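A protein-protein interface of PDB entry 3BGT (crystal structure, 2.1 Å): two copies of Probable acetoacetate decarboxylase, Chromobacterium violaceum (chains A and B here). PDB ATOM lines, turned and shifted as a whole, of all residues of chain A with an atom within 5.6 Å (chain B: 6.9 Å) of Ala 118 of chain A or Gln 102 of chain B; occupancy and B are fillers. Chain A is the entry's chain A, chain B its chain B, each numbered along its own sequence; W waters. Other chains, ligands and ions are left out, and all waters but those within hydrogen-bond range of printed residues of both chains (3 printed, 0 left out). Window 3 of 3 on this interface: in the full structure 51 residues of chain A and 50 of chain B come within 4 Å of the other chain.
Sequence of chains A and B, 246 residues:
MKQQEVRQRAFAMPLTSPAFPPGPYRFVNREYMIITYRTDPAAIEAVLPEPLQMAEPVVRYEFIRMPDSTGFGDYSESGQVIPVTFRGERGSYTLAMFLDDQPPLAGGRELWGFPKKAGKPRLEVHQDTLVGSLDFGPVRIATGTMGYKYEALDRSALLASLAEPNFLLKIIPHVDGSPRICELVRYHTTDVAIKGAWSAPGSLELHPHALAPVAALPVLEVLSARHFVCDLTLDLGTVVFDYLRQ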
ATOM      1  N   MET A  97     -23.008   4.488  14.633  1.00  0.00           N
ATOM      2  CA  MET A  97     -23.714   5.185  15.703  1.00  0.00           C
ATOM      3  C   MET A  97     -22.768   5.548  16.843  1.00  0.00           C
ATOM      4  O   MET A  97     -21.888   4.752  17.138  1.00  0.00           O
ATOM      5  CB  MET A  97     -24.868   4.329  16.229  1.00  0.00           C
ATOM      6  CG  MET A  97     -25.999   4.132  15.234  1.00  0.00           C
ATOM      7  SD  MET A  97     -27.497   3.134  15.984  1.00  0.00           S
ATOM      8  CE  MET A  97     -26.694   1.356  16.005  1.00  0.00           C
ATOM      9  N   PHE A  98     -23.274   6.470  17.484  1.00  0.00           N
ATOM     10  CA  PHE A  98     -22.553   6.971  18.672  1.00  0.00           C
ATOM     11  C   PHE A  98     -23.557   7.399  19.713  1.00  0.00           C
ATOM     12  O   PHE A  98     -24.567   8.013  19.357  1.00  0.00           O
ATOM     13  CB  PHE A  98     -21.623   8.133  18.285  1.00  0.00           C
ATOM     14  CG  PHE A  98     -20.716   7.805  17.132  1.00  0.00           C
ATOM     15  CD1 PHE A  98     -19.410   7.421  17.351  1.00  0.00           C
ATOM     16  CD2 PHE A  98     -21.194   7.813  15.818  1.00  0.00           C
ATOM     17  CE1 PHE A  98     -18.573   7.072  16.268  1.00  0.00           C
ATOM     18  CE2 PHE A  98     -20.363   7.478  14.754  1.00  0.00           C
ATOM     19  CZ  PHE A  98     -19.073   7.091  14.984  1.00  0.00           C
ATOM     20  N   LEU A  99     -23.327   7.016  20.987  1.00  0.00           N
ATOM     21  CA  LEU A  99     -24.274   7.285  22.075  1.00  0.00           C
ATOM     22  C   LEU A  99     -23.543   7.717  23.335  1.00  0.00           C
ATOM     23  O   LEU A  99     -22.381   7.391  23.500  1.00  0.00           O
ATOM     24  CB  LEU A  99     -25.029   6.023  22.514  1.00  0.00           C
ATOM     25  CG  LEU A  99     -25.508   4.847  21.714  1.00  0.00           C
ATOM     26  CD1 LEU A  99     -24.290   3.961  21.538  1.00  0.00           C
ATOM     27  CD2 LEU A  99     -26.595   4.139  22.534  1.00  0.00           C
ATOM     28  N   GLN A 102     -24.166   3.912  28.608  1.00  0.00           N
ATOM     29  CA  GLN A 102     -23.736   2.636  28.539  1.00  0.00           C
ATOM     30  C   GLN A 102     -24.641   1.532  28.280  1.00  0.00           C
ATOM     31  O   GLN A 102     -24.376   0.871  27.368  1.00  0.00           O
ATOM     32  CB  GLN A 102     -22.478   2.344  29.265  1.00  0.00           C
ATOM     33  CG  GLN A 102     -21.817   0.949  29.203  1.00  0.00           C
ATOM     34  CD  GLN A 102     -21.085   0.614  27.981  1.00  0.00           C
ATOM     35  OE1 GLN A 102     -20.900  -0.414  27.737  1.00  0.00           O
ATOM     36  NE2 GLN A 102     -20.689   1.500  27.323  1.00  0.00           N
ATOM     37  N   LEU A 105     -25.563   1.053  24.743  1.00  0.00           N
ATOM     38  CA  LEU A 105     -24.419   0.902  23.844  1.00  0.00           C
ATOM     39  C   LEU A 105     -23.978  -0.562  23.877  1.00  0.00           C
ATOM     40  O   LEU A 105     -23.849  -1.179  22.832  1.00  0.00           O
ATOM     41  CB  LEU A 105     -23.267   1.804  24.273  1.00  0.00           C
ATOM     42  CG  LEU A 105     -22.147   2.093  23.260  1.00  0.00           C
ATOM     43  CD1 LEU A 105     -21.245   3.195  23.801  1.00  0.00           C
ATOM     44  CD2 LEU A 105     -21.320   0.873  22.899  1.00  0.00           C
ATOM     45  N   ARG A 109     -25.014  -3.296  20.760  1.00  0.00           N
ATOM     46  CA  ARG A 109     -23.991  -4.191  20.204  1.00  0.00           C
ATOM     47  C   ARG A 109     -24.249  -5.693  20.475  1.00  0.00           C
ATOM     48  O   ARG A 109     -24.231  -6.494  19.546  1.00  0.00           O
ATOM     49  CB  ARG A 109     -22.599  -3.820  20.763  1.00  0.00           C
ATOM     50  CG  ARG A 109     -22.070  -2.420  20.332  1.00  0.00           C
ATOM     51  CD  ARG A 109     -20.712  -2.077  20.963  1.00  0.00           C
ATOM     52  NE  ARG A 109     -19.664  -2.970  20.460  1.00  0.00           N
ATOM     53  CZ  ARG A 109     -19.067  -2.878  19.284  1.00  0.00           C
ATOM     54  NH1 ARG A 109     -19.368  -1.910  18.442  1.00  0.00           N
ATOM     55  NH2 ARG A 109     -18.167  -3.797  18.942  1.00  0.00           N
ATOM     56  N   LYS A 116     -22.247   0.260  17.434  1.00  0.00           N
ATOM     57  CA  LYS A 116     -22.220   1.480  18.245  1.00  0.00           C
ATOM     58  C   LYS A 116     -20.871   1.791  18.847  1.00  0.00           C
ATOM     59  O   LYS A 116     -20.115   0.885  19.225  1.00  0.00           O
ATOM     60  CB  LYS A 116     -23.284   1.436  19.353  1.00  0.00           C
ATOM     61  CG  LYS A 116     -24.731   1.553  18.826  1.00  0.00           C
ATOM     62  CD  LYS A 116     -25.732   1.097  19.894  1.00  0.00           C
ATOM     63  CE  LYS A 116     -27.148   1.573  19.595  1.00  0.00           C
ATOM     64  NZ  LYS A 116     -28.132   1.079  20.639  1.00  0.00           N
ATOM     65  N   LYS A 117     -20.576   3.089  18.925  1.00  0.00           N
ATOM     66  CA  LYS A 117     -19.394   3.579  19.635  1.00  0.00           C
ATOM     67  C   LYS A 117     -19.810   4.671  20.614  1.00  0.00           C
ATOM     68  O   LYS A 117     -20.983   5.062  20.659  1.00  0.00           O
ATOM     69  CB  LYS A 117     -18.372   4.102  18.654  1.00  0.00           C
ATOM     70  CG  LYS A 117     -17.553   3.034  17.952  1.00  0.00           C
ATOM     71  CD  LYS A 117     -16.699   3.678  16.858  1.00  0.00           C
ATOM     72  CE  LYS A 117     -16.102   2.604  15.970  1.00  0.00           C
ATOM     73  NZ  LYS A 117     -15.457   3.222  14.804  1.00  0.00           N
ATOM     74  N   ALA A 118     -18.867   5.167  21.409  1.00  0.00           N
ATOM     75  CA  ALA A 118     -19.192   6.239  22.339  1.00  0.00           C
ATOM     76  C   ALA A 118     -18.985   7.598  21.695  1.00  0.00           C
ATOM     77  O   ALA A 118     -18.133   7.762  20.830  1.00  0.00           O
ATOM     78  CB  ALA A 118     -18.398   6.108  23.620  1.00  0.00           C
ATOM     79  N   GLY A 119     -19.791   8.573  22.101  1.00  0.00           N
ATOM     80  CA  GLY A 119     -19.677   9.947  21.602  1.00  0.00           C
ATOM     81  C   GLY A 119     -20.610  10.836  22.407  1.00  0.00           C
ATOM     82  O   GLY A 119     -21.348  10.336  23.276  1.00  0.00           O
ATOM     83  N   LYS A 120     -20.612  12.125  22.079  1.00  0.00           N
ATOM     84  CA  LYS A 120     -21.527  13.107  22.673  1.00  0.00           C
ATOM     85  C   LYS A 120     -22.439  13.750  21.628  1.00  0.00           C
ATOM     86  O   LYS A 120     -22.077  14.777  21.027  1.00  0.00           O
ATOM     87  CB  LYS A 120     -20.726  14.223  23.314  1.00  0.00           C
ATOM     88  CG  LYS A 120     -20.722  14.201  24.763  1.00  0.00           C
ATOM     89  CD  LYS A 120     -19.574  13.403  25.288  1.00  0.00           C
ATOM     90  CE  LYS A 120     -19.872  12.957  26.703  1.00  0.00           C
ATOM     91  NZ  LYS A 120     -21.037  12.024  26.628  1.00  0.00           N
ATOM     92  N   ASP A 135     -19.884  15.191  19.019  1.00  0.00           N
ATOM     93  CA  ASP A 135     -18.470  15.273  19.351  1.00  0.00           C
ATOM     94  C   ASP A 135     -17.978  13.858  19.656  1.00  0.00           C
ATOM     95  O   ASP A 135     -18.746  13.014  20.117  1.00  0.00           O
ATOM     96  CB  ASP A 135     -18.281  16.152  20.608  1.00  0.00           C
ATOM     97  CG  ASP A 135     -18.665  17.621  20.378  1.00  0.00           C
ATOM     98  OD1 ASP A 135     -19.391  18.173  21.215  1.00  0.00           O
ATOM     99  OD2 ASP A 135     -18.232  18.238  19.378  1.00  0.00           O
ATOM    100  N   PHE A 136     -16.698  13.615  19.389  1.00  0.00           N
ATOM    101  CA  PHE A 136     -16.008  12.402  19.781  1.00  0.00           C
ATOM    102  C   PHE A 136     -14.778  12.864  20.572  1.00  0.00           C
ATOM    103  O   PHE A 136     -13.803  13.332  20.002  1.00  0.00           O
ATOM    104  CB  PHE A 136     -15.569  11.662  18.519  1.00  0.00           C
ATOM    105  CG  PHE A 136     -15.193  10.221  18.756  1.00  0.00           C
ATOM    106  CD1 PHE A 136     -13.858   9.865  19.008  1.00  0.00           C
ATOM    107  CD2 PHE A 136     -16.169   9.205  18.716  1.00  0.00           C
ATOM    108  CE1 PHE A 136     -13.494   8.525  19.215  1.00  0.00           C
ATOM    109  CE2 PHE A 136     -15.814   7.861  18.904  1.00  0.00           C
ATOM    110  CZ  PHE A 136     -14.479   7.520  19.186  1.00  0.00           C
ATOM    111  N   ALA B  19     -14.504  -1.365  16.754  1.00  0.00           N
ATOM    112  CA  ALA B  19     -14.615  -0.566  17.957  1.00  0.00           C
ATOM    113  C   ALA B  19     -13.390  -0.715  18.839  1.00  0.00           C
ATOM    114  O   ALA B  19     -13.177   0.082  19.750  1.00  0.00           O
ATOM    115  CB  ALA B  19     -15.867  -0.926  18.698  1.00  0.00           C
ATOM    116  N   PHE B  20     -12.609  -1.755  18.552  1.00  0.00           N
ATOM    117  CA  PHE B  20     -11.332  -2.044  19.185  1.00  0.00           C
ATOM    118  C   PHE B  20     -10.520  -2.910  18.216  1.00  0.00           C
ATOM    119  O   PHE B  20     -11.096  -3.722  17.479  1.00  0.00           O
ATOM    120  CB  PHE B  20     -11.522  -2.789  20.521  1.00  0.00           C
ATOM    121  CG  PHE B  20     -12.442  -3.985  20.433  1.00  0.00           C
ATOM    122  CD1 PHE B  20     -11.920  -5.274  20.254  1.00  0.00           C
ATOM    123  CD2 PHE B  20     -13.832  -3.823  20.520  1.00  0.00           C
ATOM    124  CE1 PHE B  20     -12.782  -6.404  20.152  1.00  0.00           C
ATOM    125  CE2 PHE B  20     -14.705  -4.919  20.412  1.00  0.00           C
ATOM    126  CZ  PHE B  20     -14.184  -6.223  20.259  1.00  0.00           C
ATOM    127  N   PHE B  72      -6.099   0.603  23.099  1.00  0.00           N
ATOM    128  CA  PHE B  72      -7.150   1.057  24.030  1.00  0.00           C
ATOM    129  C   PHE B  72      -6.975   2.507  24.487  1.00  0.00           C
ATOM    130  O   PHE B  72      -7.953   3.235  24.630  1.00  0.00           O
ATOM    131  CB  PHE B  72      -7.213   0.155  25.271  1.00  0.00           C
ATOM    132  CG  PHE B  72      -7.672  -1.247  24.989  1.00  0.00           C
ATOM    133  CD1 PHE B  72      -8.604  -1.509  23.979  1.00  0.00           C
ATOM    134  CD2 PHE B  72      -7.192  -2.320  25.755  1.00  0.00           C
ATOM    135  CE1 PHE B  72      -9.055  -2.816  23.726  1.00  0.00           C
ATOM    136  CE2 PHE B  72      -7.626  -3.626  25.496  1.00  0.00           C
ATOM    137  CZ  PHE B  72      -8.562  -3.869  24.472  1.00  0.00           C
ATOM    138  N   LEU B  99     -14.927   0.991  33.961  1.00  0.00           N
ATOM    139  CA  LEU B  99     -13.878   1.723  33.215  1.00  0.00           C
ATOM    140  C   LEU B  99     -14.438   2.993  32.609  1.00  0.00           C
ATOM    141  O   LEU B  99     -15.648   3.058  32.335  1.00  0.00           O
ATOM    142  CB  LEU B  99     -13.360   0.948  32.011  1.00  0.00           C
ATOM    143  CG  LEU B  99     -13.043  -0.517  31.884  1.00  0.00           C
ATOM    144  CD1 LEU B  99     -14.391  -1.192  31.850  1.00  0.00           C
ATOM    145  CD2 LEU B  99     -12.297  -0.745  30.580  1.00  0.00           C
ATOM    146  N   ASP B 100     -13.526   3.928  32.304  1.00  0.00           N
ATOM    147  CA  ASP B 100     -13.847   5.234  31.719  1.00  0.00           C
ATOM    148  C   ASP B 100     -13.413   5.404  30.239  1.00  0.00           C
ATOM    149  O   ASP B 100     -13.099   6.516  29.801  1.00  0.00           O
ATOM    150  CB  ASP B 100     -13.249   6.372  32.584  1.00  0.00           C
ATOM    151  CG  ASP B 100     -11.702   6.310  32.704  1.00  0.00           C
ATOM    152  OD1 ASP B 100     -11.123   7.171  33.409  1.00  0.00           O
ATOM    153  OD2 ASP B 100     -11.051   5.452  32.070  1.00  0.00           O
ATOM    154  N   ASP B 101     -13.392   4.326  29.467  1.00  0.00           N
ATOM    155  CA  ASP B 101     -12.888   4.402  28.102  1.00  0.00           C
ATOM    156  C   ASP B 101     -13.599   3.243  27.388  1.00  0.00           C
ATOM    157  O   ASP B 101     -13.649   2.127  27.951  1.00  0.00           O
ATOM    158  CB  ASP B 101     -11.348   4.282  28.155  1.00  0.00           C
ATOM    159  CG  ASP B 101     -10.634   4.381  26.790  1.00  0.00           C
ATOM    160  OD1 ASP B 101     -11.165   4.867  25.743  1.00  0.00           O
ATOM    161  OD2 ASP B 101      -9.460   3.939  26.781  1.00  0.00           O
ATOM    162  N   GLN B 102     -14.171   3.522  26.204  1.00  0.00           N
ATOM    163  CA  GLN B 102     -15.099   2.606  25.514  1.00  0.00           C
ATOM    164  C   GLN B 102     -14.413   1.426  24.849  1.00  0.00           C
ATOM    165  O   GLN B 102     -14.806   0.281  25.116  1.00  0.00           O
ATOM    166  CB  GLN B 102     -16.000   3.346  24.499  1.00  0.00           C
ATOM    167  CG  GLN B 102     -16.986   2.435  23.683  1.00  0.00           C
ATOM    168  CD  GLN B 102     -17.920   1.562  24.546  1.00  0.00           C
ATOM    169  OE1 GLN B 102     -18.240   1.898  25.690  1.00  0.00           O
ATOM    170  NE2 GLN B 102     -18.397   0.470  23.970  1.00  0.00           N
ATOM    171  N   PRO B 103     -13.359   1.679  24.032  1.00  0.00           N
ATOM    172  CA  PRO B 103     -12.698   0.539  23.380  1.00  0.00           C
ATOM    173  C   PRO B 103     -12.322  -0.597  24.310  1.00  0.00           C
ATOM    174  O   PRO B 103     -12.586  -1.754  23.955  1.00  0.00           O
ATOM    175  CB  PRO B 103     -11.445   1.163  22.737  1.00  0.00           C
ATOM    176  CG  PRO B 103     -11.804   2.588  22.524  1.00  0.00           C
ATOM    177  CD  PRO B 103     -12.729   2.967  23.643  1.00  0.00           C
ATOM    178  N   PRO B 104     -11.676  -0.302  25.488  1.00  0.00           N
ATOM    179  CA  PRO B 104     -11.420  -1.457  26.358  1.00  0.00           C
ATOM    180  C   PRO B 104     -12.645  -2.049  27.036  1.00  0.00           C
ATOM    181  O   PRO B 104     -12.565  -3.165  27.556  1.00  0.00           O
ATOM    182  CB  PRO B 104     -10.440  -0.912  27.401  1.00  0.00           C
ATOM    183  CG  PRO B 104     -10.706   0.581  27.428  1.00  0.00           C
ATOM    184  CD  PRO B 104     -11.078   0.938  26.024  1.00  0.00           C
ATOM    185  N   LEU B 105     -13.736  -1.295  27.088  1.00  0.00           N
ATOM    186  CA  LEU B 105     -14.975  -1.770  27.694  1.00  0.00           C
ATOM    187  C   LEU B 105     -15.654  -2.749  26.729  1.00  0.00           C
ATOM    188  O   LEU B 105     -15.883  -3.900  27.078  1.00  0.00           O
ATOM    189  CB  LEU B 105     -15.879  -0.584  28.014  1.00  0.00           C
ATOM    190  CG  LEU B 105     -16.864  -0.638  29.200  1.00  0.00           C
ATOM    191  CD1 LEU B 105     -17.522   0.738  29.350  1.00  0.00           C
ATOM    192  CD2 LEU B 105     -17.917  -1.672  29.002  1.00  0.00           C
ATOM    193  N   ALA B 106     -15.936  -2.312  25.509  1.00  0.00           N
ATOM    194  CA  ALA B 106     -16.439  -3.196  24.482  1.00  0.00           C
ATOM    195  C   ALA B 106     -15.493  -4.352  24.237  1.00  0.00           C
ATOM    196  O   ALA B 106     -15.920  -5.476  24.240  1.00  0.00           O
ATOM    197  CB  ALA B 106     -16.669  -2.441  23.158  1.00  0.00           C
ATOM    198  N   GLY B 107     -14.214  -4.055  24.009  1.00  0.00           N
ATOM    199  CA  GLY B 107     -13.224  -5.102  23.784  1.00  0.00           C
ATOM    200  C   GLY B 107     -13.108  -6.094  24.917  1.00  0.00           C
ATOM    201  O   GLY B 107     -13.085  -7.288  24.672  1.00  0.00           O
ATOM    202  N   GLY B 108     -13.000  -5.602  26.150  1.00  0.00           N
ATOM    203  CA  GLY B 108     -13.009  -6.473  27.335  1.00  0.00           C
ATOM    204  C   GLY B 108     -14.196  -7.440  27.344  1.00  0.00           C
ATOM    205  O   GLY B 108     -14.033  -8.672  27.553  1.00  0.00           O
ATOM    206  N   GLU B 110     -16.432  -8.187  24.739  1.00  0.00           N
ATOM    207  CA  GLU B 110     -16.806  -8.985  23.568  1.00  0.00           C
ATOM    208  C   GLU B 110     -15.753 -10.032  23.216  1.00  0.00           C
ATOM    209  O   GLU B 110     -16.086 -11.090  22.646  1.00  0.00           O
ATOM    210  CB  GLU B 110     -17.117  -8.102  22.361  1.00  0.00           C
ATOM    211  CG  GLU B 110     -18.301  -7.156  22.590  1.00  0.00           C
ATOM    212  CD  GLU B 110     -18.367  -6.002  21.586  1.00  0.00           C
ATOM    213  OE1 GLU B 110     -17.729  -6.073  20.504  1.00  0.00           O
ATOM    214  OE2 GLU B 110     -19.033  -5.001  21.893  1.00  0.00           O
ATOM    215  N   ALA B 118     -19.590   0.964  32.750  1.00  0.00           N
ATOM    216  CA  ALA B 118     -18.987   2.304  32.732  1.00  0.00           C
ATOM    217  C   ALA B 118     -18.909   2.806  34.171  1.00  0.00           C
ATOM    218  O   ALA B 118     -19.724   2.410  35.002  1.00  0.00           O
ATOM    219  CB  ALA B 118     -19.833   3.255  31.880  1.00  0.00           C
HETATM  220  O   HOH W   1     -19.799  -1.665  25.322  1.00  0.00           O
HETATM  221  O   HOH W   2     -17.824  -6.768  18.085  1.00  0.00           O
HETATM  222  O   HOH W   3     -18.009   0.491  21.215  1.00  0.00           O
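The side-chain amide nitrogen (NE2) of Gln 102 of chain A sits at hydrogen-bond distance from the side-chain amide oxygen (OE1) of Gln 102 of chain B, 3.0 Å away.
The guanidinium group (NE) of Arg 109 of chain A is in salt-bridge range of the side-chain carboxylate (OE2) of Glu 110 of chain B (2.6 Å).
NH1 of Arg 109 of chain A is in hydrogen-bond range of O of Lys 116 of chain A, at 3.0 Å.
Among the printed residues, merely in contact across the chains: Gln 102 of chain A with Leu 105 of chain B (3.5 Å), Gln 102 of chain A with Ala 118 of chain B (3.8 Å), Leu 105 of chain A with Gln 102 of chain B (3.1 Å), Arg 109 of chain A with Ala 19 of chain B (3.6 Å), Arg 109 of chain A with Phe 20 of chain B (3.9 Å) and Ala 118 of chain A with Gln 102 of chain B (3.8 Å).
Printed residues of chain B within 4 Å of Gln 102 of chain A: Gln 102, Leu 105 and Ala 118.
Printed residues of chain B within 4 Å of Arg 109 of chain A: Ala 19 (3.6 Å), Phe 20 (3.9 Å) and Glu 110 (2.6 Å).
Of chain B, only Gln 102 comes within 4 Å of Ala 118 of chain A.
Of the printed residues of chain A, Phe 20 of chain B touches Arg 109 (3.9 Å).
Phe 72 of chain B touches none of the printed residues of chain A.
Gln 102 of chain B touches just these residues of chain A: Gln 102, Leu 105 and Ala 118.
Of the printed residues of chain A, Ala 118 of chain B touches Gln 102.
The nearest residue of chain B that does not touch Ala 118 of chain A is Pro 103 of chain B (6.5 Å).
The nearest residue of chain A that does not touch Gln 102 of chain B is Arg 109 of chain A (4.6 Å).
The nearest printed residue of chain A that does not touch Glu 110 of chain B is Leu 105 of chain A (6.2 Å).
Of the 15 printed residues of chain B, 6 touch a printed residue of chain A.
Printed residues of chain A that touch a printed residue of chain B: Gln 102, Leu 105, Arg 109 and Ala 118.
Gln 102 of chain A touches its own counterpart, Gln 102 of chain B.
Gln 102 of chain A touches Leu 105 of chain B, and with the chains exchanged Leu 105 of chain A touches Gln 102 of chain B.
Gln 102 of chain A touches Ala 118 of chain B, and with the chains exchanged Ala 118 of chain A touches Gln 102 of chain B.
Of the 8 pairs that touch across the chains among the printed residues, 5 have their exchanged pair printed and touching as well.
Water W2 bridges the side-chain carboxylate of Glu 110 of chain B and the guanidinium group of Arg 109 of chain A.
Water W3 lies within hydrogen-bond range of NE2 of Gln 102 of chain B (2.8 Å) and O of Lys 116 of chain A (2.9 Å).
Water W1 lies within hydrogen-bond range of NE2 of Gln 102 of chain B and OE1 of Gln 102 of chain A.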
